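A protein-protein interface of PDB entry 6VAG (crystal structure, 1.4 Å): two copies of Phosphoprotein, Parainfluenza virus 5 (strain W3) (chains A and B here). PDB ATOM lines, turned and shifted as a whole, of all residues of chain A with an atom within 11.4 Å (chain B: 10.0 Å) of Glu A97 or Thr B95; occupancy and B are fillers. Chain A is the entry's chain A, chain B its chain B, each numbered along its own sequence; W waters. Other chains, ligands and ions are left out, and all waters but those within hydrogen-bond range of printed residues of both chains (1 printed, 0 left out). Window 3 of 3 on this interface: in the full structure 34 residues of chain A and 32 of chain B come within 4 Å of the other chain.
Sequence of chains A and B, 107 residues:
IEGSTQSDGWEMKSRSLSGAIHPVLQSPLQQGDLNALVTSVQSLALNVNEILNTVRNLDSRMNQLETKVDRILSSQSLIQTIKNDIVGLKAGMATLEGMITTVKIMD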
ATOM      1  N   GLY A  88      24.700  21.281  15.586  1.00  0.00           N
ATOM      2  CA  GLY A  88      24.680  22.632  16.124  1.00  0.00           C
ATOM      3  C   GLY A  88      24.207  22.676  17.564  1.00  0.00           C
ATOM      4  O   GLY A  88      24.786  23.377  18.400  1.00  0.00           O
ATOM      5  N   LEU A  89      23.141  21.935  17.874  1.00  0.00           N
ATOM      6  CA  LEU A  89      22.692  21.835  19.259  1.00  0.00           C
ATOM      7  C   LEU A  89      23.790  21.276  20.155  1.00  0.00           C
ATOM      8  O   LEU A  89      23.915  21.683  21.318  1.00  0.00           O
ATOM      9  CB  LEU A  89      21.439  20.961  19.332  1.00  0.00           C
ATOM     10  CG  LEU A  89      20.159  21.553  18.736  1.00  0.00           C
ATOM     11  CD1 LEU A  89      19.062  20.494  18.654  1.00  0.00           C
ATOM     12  CD2 LEU A  89      19.693  22.756  19.548  1.00  0.00           C
ATOM     13  N   LYS A  90      24.604  20.360  19.628  1.00  0.00           N
ATOM     14  CA  LYS A  90      25.697  19.788  20.404  1.00  0.00           C
ATOM     15  C   LYS A  90      26.723  20.853  20.780  1.00  0.00           C
ATOM     16  O   LYS A  90      27.077  21.003  21.955  1.00  0.00           O
ATOM     17  CB  LYS A  90      26.352  18.661  19.606  1.00  0.00           C
ATOM     18  CG  LYS A  90      27.079  17.638  20.450  1.00  0.00           C
ATOM     19  CD  LYS A  90      26.901  16.237  19.886  1.00  0.00           C
ATOM     20  CE  LYS A  90      27.464  16.124  18.473  1.00  0.00           C
ATOM     21  NZ  LYS A  90      28.955  16.134  18.483  1.00  0.00           N
ATOM     22  N   ALA A  91      27.224  21.594  19.785  1.00  0.00           N
ATOM     23  CA  ALA A  91      28.180  22.658  20.067  1.00  0.00           C
ATOM     24  C   ALA A  91      27.589  23.701  21.000  1.00  0.00           C
ATOM     25  O   ALA A  91      28.304  24.270  21.833  1.00  0.00           O
ATOM     26  CB  ALA A  91      28.643  23.318  18.766  1.00  0.00           C
ATOM     27  N   GLY A  92      26.290  23.969  20.876  1.00  0.00           N
ATOM     28  CA  GLY A  92      25.668  24.922  21.780  1.00  0.00           C
ATOM     29  C   GLY A  92      25.671  24.436  23.217  1.00  0.00           C
ATOM     30  O   GLY A  92      26.110  25.148  24.126  1.00  0.00           O
ATOM     31  N   MET A  93      25.143  23.230  23.448  1.00  0.00           N
ATOM     32  CA  MET A  93      25.048  22.717  24.813  1.00  0.00           C
ATOM     33  C   MET A  93      26.416  22.678  25.480  1.00  0.00           C
ATOM     34  O   MET A  93      26.536  22.926  26.686  1.00  0.00           O
ATOM     35  CB  MET A  93      24.380  21.337  24.819  1.00  0.00           C
ATOM     36  CG  MET A  93      23.984  20.825  26.201  1.00  0.00           C
ATOM     37  SD  MET A  93      22.824  19.441  26.111  1.00  0.00           S
ATOM     38  CE  MET A  93      21.527  20.144  25.094  1.00  0.00           C
ATOM     39  N   ALA A  94      27.463  22.372  24.709  1.00  0.00           N
ATOM     40  CA  ALA A  94      28.816  22.491  25.237  1.00  0.00           C
ATOM     41  C   ALA A  94      29.123  23.932  25.616  1.00  0.00           C
ATOM     42  O   ALA A  94      29.790  24.190  26.624  1.00  0.00           O
ATOM     43  CB  ALA A  94      29.830  21.983  24.213  1.00  0.00           C
ATOM     44  N   THR A  95      28.637  24.888  24.819  1.00  0.00           N
ATOM     45  CA  THR A  95      28.835  26.294  25.149  1.00  0.00           C
ATOM     46  C   THR A  95      28.180  26.644  26.480  1.00  0.00           C
ATOM     47  O   THR A  95      28.767  27.357  27.303  1.00  0.00           O
ATOM     48  CB  THR A  95      28.288  27.171  24.024  1.00  0.00           C
ATOM     49  OG1 THR A  95      29.020  26.908  22.821  1.00  0.00           O
ATOM     50  CG2 THR A  95      28.420  28.649  24.379  1.00  0.00           C
ATOM     51  N   LEU A  96      26.960  26.151  26.710  1.00  0.00           N
ATOM     52  CA  LEU A  96      26.300  26.389  27.990  1.00  0.00           C
ATOM     53  C   LEU A  96      27.139  25.845  29.140  1.00  0.00           C
ATOM     54  O   LEU A  96      27.388  26.545  30.129  1.00  0.00           O
ATOM     55  CB  LEU A  96      24.908  25.756  27.985  1.00  0.00           C
ATOM     56  CG  LEU A  96      23.955  26.206  26.875  1.00  0.00           C
ATOM     57  CD1 LEU A  96      22.522  25.822  27.212  1.00  0.00           C
ATOM     58  CD2 LEU A  96      24.073  27.706  26.642  1.00  0.00           C
ATOM     59  N   GLU A  97      27.592  24.596  29.022  1.00  0.00           N
ATOM     60  CA  GLU A  97      28.421  24.011  30.072  1.00  0.00           C
ATOM     61  C   GLU A  97      29.728  24.778  30.232  1.00  0.00           C
ATOM     62  O   GLU A  97      30.185  25.015  31.357  1.00  0.00           O
ATOM     63  CB  GLU A  97      28.695  22.539  29.764  1.00  0.00           C
ATOM     64  CG  GLU A  97      27.484  21.775  29.263  1.00  0.00           C
ATOM     65  CD  GLU A  97      27.699  20.274  29.275  1.00  0.00           C
ATOM     66  OE1 GLU A  97      28.476  19.792  30.128  1.00  0.00           O
ATOM     67  OE2 GLU A  97      27.094  19.577  28.435  1.00  0.00           O
ATOM     68  N   GLY A  98      30.345  25.172  29.116  1.00  0.00           N
ATOM     69  CA  GLY A  98      31.593  25.914  29.196  1.00  0.00           C
ATOM     70  C   GLY A  98      31.432  27.248  29.899  1.00  0.00           C
ATOM     71  O   GLY A  98      32.276  27.641  30.709  1.00  0.00           O
ATOM     72  N   MET A  99      30.347  27.965  29.598  1.00  0.00           N
ATOM     73  CA  MET A  99      30.080  29.212  30.304  1.00  0.00           C
ATOM     74  C   MET A  99      29.811  28.966  31.781  1.00  0.00           C
ATOM     75  O   MET A  99      30.148  29.810  32.621  1.00  0.00           O
ATOM     76  CB  MET A  99      28.918  29.953  29.646  1.00  0.00           C
ATOM     77  CG  MET A  99      29.158  30.273  28.180  1.00  0.00           C
ATOM     78  SD  MET A  99      28.014  31.501  27.522  1.00  0.00           S
ATOM     79  CE  MET A  99      26.493  30.553  27.479  1.00  0.00           C
ATOM     80  N   ILE A 100      29.218  27.825  32.116  1.00  0.00           N
ATOM     81  CA  ILE A 100      29.024  27.438  33.508  1.00  0.00           C
ATOM     82  C   ILE A 100      27.994  28.329  34.191  1.00  0.00           C
ATOM     83  O   ILE A 100      26.795  28.211  33.936  1.00  0.00           O
ATOM     84  CB  ILE A 100      30.365  27.415  34.272  1.00  0.00           C
ATOM     85  CG1 ILE A 100      31.137  26.130  33.960  1.00  0.00           C
ATOM     86  CG2 ILE A 100      30.133  27.562  35.765  1.00  0.00           C
ATOM     87  CD1 ILE A 100      32.555  26.123  34.494  1.00  0.00           C
ATOM     88  N   VAL B  87      22.227  10.869  22.056  1.00  0.00           N
ATOM     89  CA  VAL B  87      22.656  10.270  23.319  1.00  0.00           C
ATOM     90  C   VAL B  87      23.501  11.260  24.108  1.00  0.00           C
ATOM     91  O   VAL B  87      23.305  11.453  25.316  1.00  0.00           O
ATOM     92  CB  VAL B  87      23.407   8.949  23.070  1.00  0.00           C
ATOM     93  CG1 VAL B  87      24.027   8.437  24.367  1.00  0.00           C
ATOM     94  CG2 VAL B  87      22.472   7.910  22.478  1.00  0.00           C
ATOM     95  N   GLY B  88      24.456  11.904  23.435  1.00  0.00           N
ATOM     96  CA  GLY B  88      25.262  12.911  24.105  1.00  0.00           C
ATOM     97  C   GLY B  88      24.446  14.108  24.551  1.00  0.00           C
ATOM     98  O   GLY B  88      24.671  14.657  25.632  1.00  0.00           O
ATOM     99  N   LEU B  89      23.482  14.528  23.726  1.00  0.00           N
ATOM    100  CA  LEU B  89      22.633  15.659  24.095  1.00  0.00           C
ATOM    101  C   LEU B  89      21.822  15.353  25.348  1.00  0.00           C
ATOM    102  O   LEU B  89      21.632  16.224  26.204  1.00  0.00           O
ATOM    103  CB  LEU B  89      21.708  16.019  22.931  1.00  0.00           C
ATOM    104  CG  LEU B  89      22.396  16.630  21.712  1.00  0.00           C
ATOM    105  CD1 LEU B  89      21.366  17.019  20.662  1.00  0.00           C
ATOM    106  CD2 LEU B  89      23.238  17.833  22.123  1.00  0.00           C
ATOM    107  N   LYS B  90      21.329  14.119  25.467  1.00  0.00           N
ATOM    108  CA  LYS B  90      20.598  13.727  26.664  1.00  0.00           C
ATOM    109  C   LYS B  90      21.502  13.756  27.888  1.00  0.00           C
ATOM    110  O   LYS B  90      21.091  14.202  28.966  1.00  0.00           O
ATOM    111  CB  LYS B  90      20.012  12.329  26.473  1.00  0.00           C
ATOM    112  CG  LYS B  90      19.093  12.199  25.275  1.00  0.00           C
ATOM    113  CD  LYS B  90      17.668  11.887  25.706  1.00  0.00           C
ATOM    114  CE  LYS B  90      17.461  10.388  25.880  1.00  0.00           C
ATOM    115  NZ  LYS B  90      16.060  10.052  26.268  1.00  0.00           N
ATOM    116  N   ALA B  91      22.741  13.279  27.741  1.00  0.00           N
ATOM    117  CA  ALA B  91      23.660  13.242  28.874  1.00  0.00           C
ATOM    118  C   ALA B  91      24.119  14.642  29.251  1.00  0.00           C
ATOM    119  O   ALA B  91      24.010  15.052  30.414  1.00  0.00           O
ATOM    120  CB  ALA B  91      24.861  12.353  28.550  1.00  0.00           C
ATOM    121  N   GLY B  92      24.649  15.390  28.280  1.00  0.00           N
ATOM    122  CA  GLY B  92      25.067  16.751  28.559  1.00  0.00           C
ATOM    123  C   GLY B  92      23.963  17.584  29.172  1.00  0.00           C
ATOM    124  O   GLY B  92      24.231  18.510  29.944  1.00  0.00           O
ATOM    125  N   MET B  93      22.709  17.260  28.858  1.00  0.00           N
ATOM    126  CA  MET B  93      21.602  18.041  29.385  1.00  0.00           C
ATOM    127  C   MET B  93      21.252  17.657  30.816  1.00  0.00           C
ATOM    128  O   MET B  93      20.844  18.521  31.600  1.00  0.00           O
ATOM    129  CB  MET B  93      20.377  17.905  28.493  1.00  0.00           C
ATOM    130  CG  MET B  93      19.355  18.942  28.821  1.00  0.00           C
ATOM    131  SD  MET B  93      17.690  18.300  28.761  1.00  0.00           S
ATOM    132  CE  MET B  93      16.874  19.792  29.268  1.00  0.00           C
ATOM    133  N   ALA B  94      21.381  16.376  31.170  1.00  0.00           N
ATOM    134  CA  ALA B  94      21.280  15.999  32.575  1.00  0.00           C
ATOM    135  C   ALA B  94      22.299  16.768  33.404  1.00  0.00           C
ATOM    136  O   ALA B  94      22.034  17.132  34.556  1.00  0.00           O
ATOM    137  CB  ALA B  94      21.476  14.492  32.730  1.00  0.00           C
ATOM    138  N   THR B  95      23.474  17.027  32.826  1.00  0.00           N
ATOM    139  CA  THR B  95      24.454  17.887  33.480  1.00  0.00           C
ATOM    140  C   THR B  95      23.877  19.275  33.732  1.00  0.00           C
ATOM    141  O   THR B  95      23.929  19.788  34.855  1.00  0.00           O
ATOM    142  CB  THR B  95      25.713  17.977  32.616  1.00  0.00           C
ATOM    143  OG1 THR B  95      26.312  16.680  32.498  1.00  0.00           O
ATOM    144  CG2 THR B  95      26.715  18.949  33.227  1.00  0.00           C
ATOM    145  N   LEU B  96      23.317  19.898  32.691  1.00  0.00           N
ATOM    146  CA  LEU B  96      22.743  21.231  32.853  1.00  0.00           C
ATOM    147  C   LEU B  96      21.632  21.227  33.893  1.00  0.00           C
ATOM    148  O   LEU B  96      21.549  22.138  34.727  1.00  0.00           O
ATOM    149  CB  LEU B  96      22.224  21.749  31.511  1.00  0.00           C
ATOM    150  CG  LEU B  96      23.230  22.474  30.615  1.00  0.00           C
ATOM    151  CD1 LEU B  96      24.608  21.847  30.743  1.00  0.00           C
ATOM    152  CD2 LEU B  96      22.763  22.449  29.166  1.00  0.00           C
ATOM    153  N   GLU B  97      20.770  20.208  33.863  1.00  0.00           N
ATOM    154  CA  GLU B  97      19.717  20.105  34.867  1.00  0.00           C
ATOM    155  C   GLU B  97      20.302  20.039  36.273  1.00  0.00           C
ATOM    156  O   GLU B  97      19.742  20.613  37.214  1.00  0.00           O
ATOM    157  CB  GLU B  97      18.837  18.886  34.588  1.00  0.00           C
ATOM    158  CG  GLU B  97      18.088  18.959  33.266  1.00  0.00           C
ATOM    159  CD  GLU B  97      16.594  18.759  33.428  1.00  0.00           C
ATOM    160  OE1 GLU B  97      16.108  17.637  33.173  1.00  0.00           O
ATOM    161  OE2 GLU B  97      15.906  19.727  33.819  1.00  0.00           O
ATOM    162  N   GLY B  98      21.428  19.343  36.435  1.00  0.00           N
ATOM    163  CA  GLY B  98      22.087  19.324  37.731  1.00  0.00           C
ATOM    164  C   GLY B  98      22.573  20.699  38.143  1.00  0.00           C
ATOM    165  O   GLY B  98      22.348  21.141  39.274  1.00  0.00           O
ATOM    166  N   MET B  99      23.245  21.395  37.232  1.00  0.00           N
ATOM    167  CA  MET B  99      23.720  22.746  37.496  1.00  0.00           C
ATOM    168  C   MET B  99      22.544  23.709  37.622  1.00  0.00           C
ATOM    169  O   MET B  99      22.458  24.477  38.581  1.00  0.00           O
ATOM    170  CB  MET B  99      24.664  23.210  36.383  1.00  0.00           C
ATOM    171  CG  MET B  99      25.758  22.208  36.037  1.00  0.00           C
ATOM    172  SD  MET B  99      26.577  22.562  34.467  1.00  0.00           S
ATOM    173  CE  MET B  99      28.135  21.706  34.698  1.00  0.00           C
HETATM  174  O   HOH W   1      27.613  17.055  30.208  1.00  0.00           O
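The side-chain sulfur (SD) of Met A93 sits at hydrogen-bond distance from the backbone NH (N) of Met B93.
The side-chain sulfur (SD) of Met A93 sits close to the backbone carbonyl oxygen (O) of Leu B89, at 3.4 Å.
O of Gly B92 lies close to OE2 of Glu A97 (3.4 Å).
Among the printed residues, merely in contact across the chains: Glu A97 with Leu B96, Lys A90 with Leu B89, Met A93 with Leu B96, Glu A97 with Thr B95, Met A93 with Gly B92, Leu A96 with Leu B96 and Leu A89 with Leu B89.
Glu A97 touches just these residues of chain B: Gly B92 (3.4 Å), Thr B95 (3.7 Å) and Leu B96 (3.2 Å).
Thr B95 touches one residue of chain A.
No residue of chain B comes within 4 Å of Ala A94.
No residue of chain B comes within 4 Å of Gly A98.
No residue of chain B comes within 4 Å of Ile A100.
Gly B92 touches just these residues of chain A: Met A93 and Glu A97.
Leu B96 touches just these residues of chain A: Met A93 (3.6 Å), Leu A96 (3.9 Å) and Glu A97 (3.2 Å).
No residue of chain A comes within 4 Å of Met B99.
Of the printed residues of chain B, Lys A90 touches Leu B89 (3.6 Å).
Printed residues of chain B within 4 Å of Leu A89: Leu B89 (3.99 Å).
Of the printed residues of chain A, Leu B89 touches Leu A89 (3.99 Å), Lys A90 (3.6 Å) and Met A93 (3.4 Å).
Printed residues of chain B within 4 Å of Met A93: Leu B89, Gly B92, Met B93 and Leu B96.
Gly A88 touches none of the printed residues of chain B.
The nearest printed residue of chain B that does not touch Glu A97 is Met B99 (5.0 Å).
The nearest printed residue of chain B that does not touch Leu A89 is Leu B96 (8.0 Å).
Of the 13 printed residues of chain B, 5 touch a printed residue of chain A.
Printed residues of chain B that touch a printed residue of chain A: Leu B89, Gly B92, Met B93, Thr B95 and Leu B96.
Hydrophobic or aromatic side chains of chain B within 4 Å of the printed part of chain A: Leu B89, Met B93 and Leu B96.
Among the printed residues, 10 pairs touch across the chains.
Among the printed residues, no Asp or Glu carboxylate lies within 4 Å of a Lys or Arg side-chain nitrogen of the other chain.
Lys A90 touches Leu B89, but with the chains exchanged Leu A89 does not touch Lys B90 (9.0 Å).
Met A93 touches Gly B92, but with the chains exchanged Gly A92 does not touch Met B93 (9.6 Å).
Met A93 touches Leu B96, but with the chains exchanged Leu A96 does not touch Met B93 (7.7 Å).
Leu A96 touches its own counterpart, Leu B96.
Of the 10 pairs that touch across the chains among the printed residues, 3 have their exchanged pair printed and touching as well.
Water W1 bridges the side-chain hydroxyl (OG1) of Thr B95 and the side-chain carboxylate (OE1) of Glu A97.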
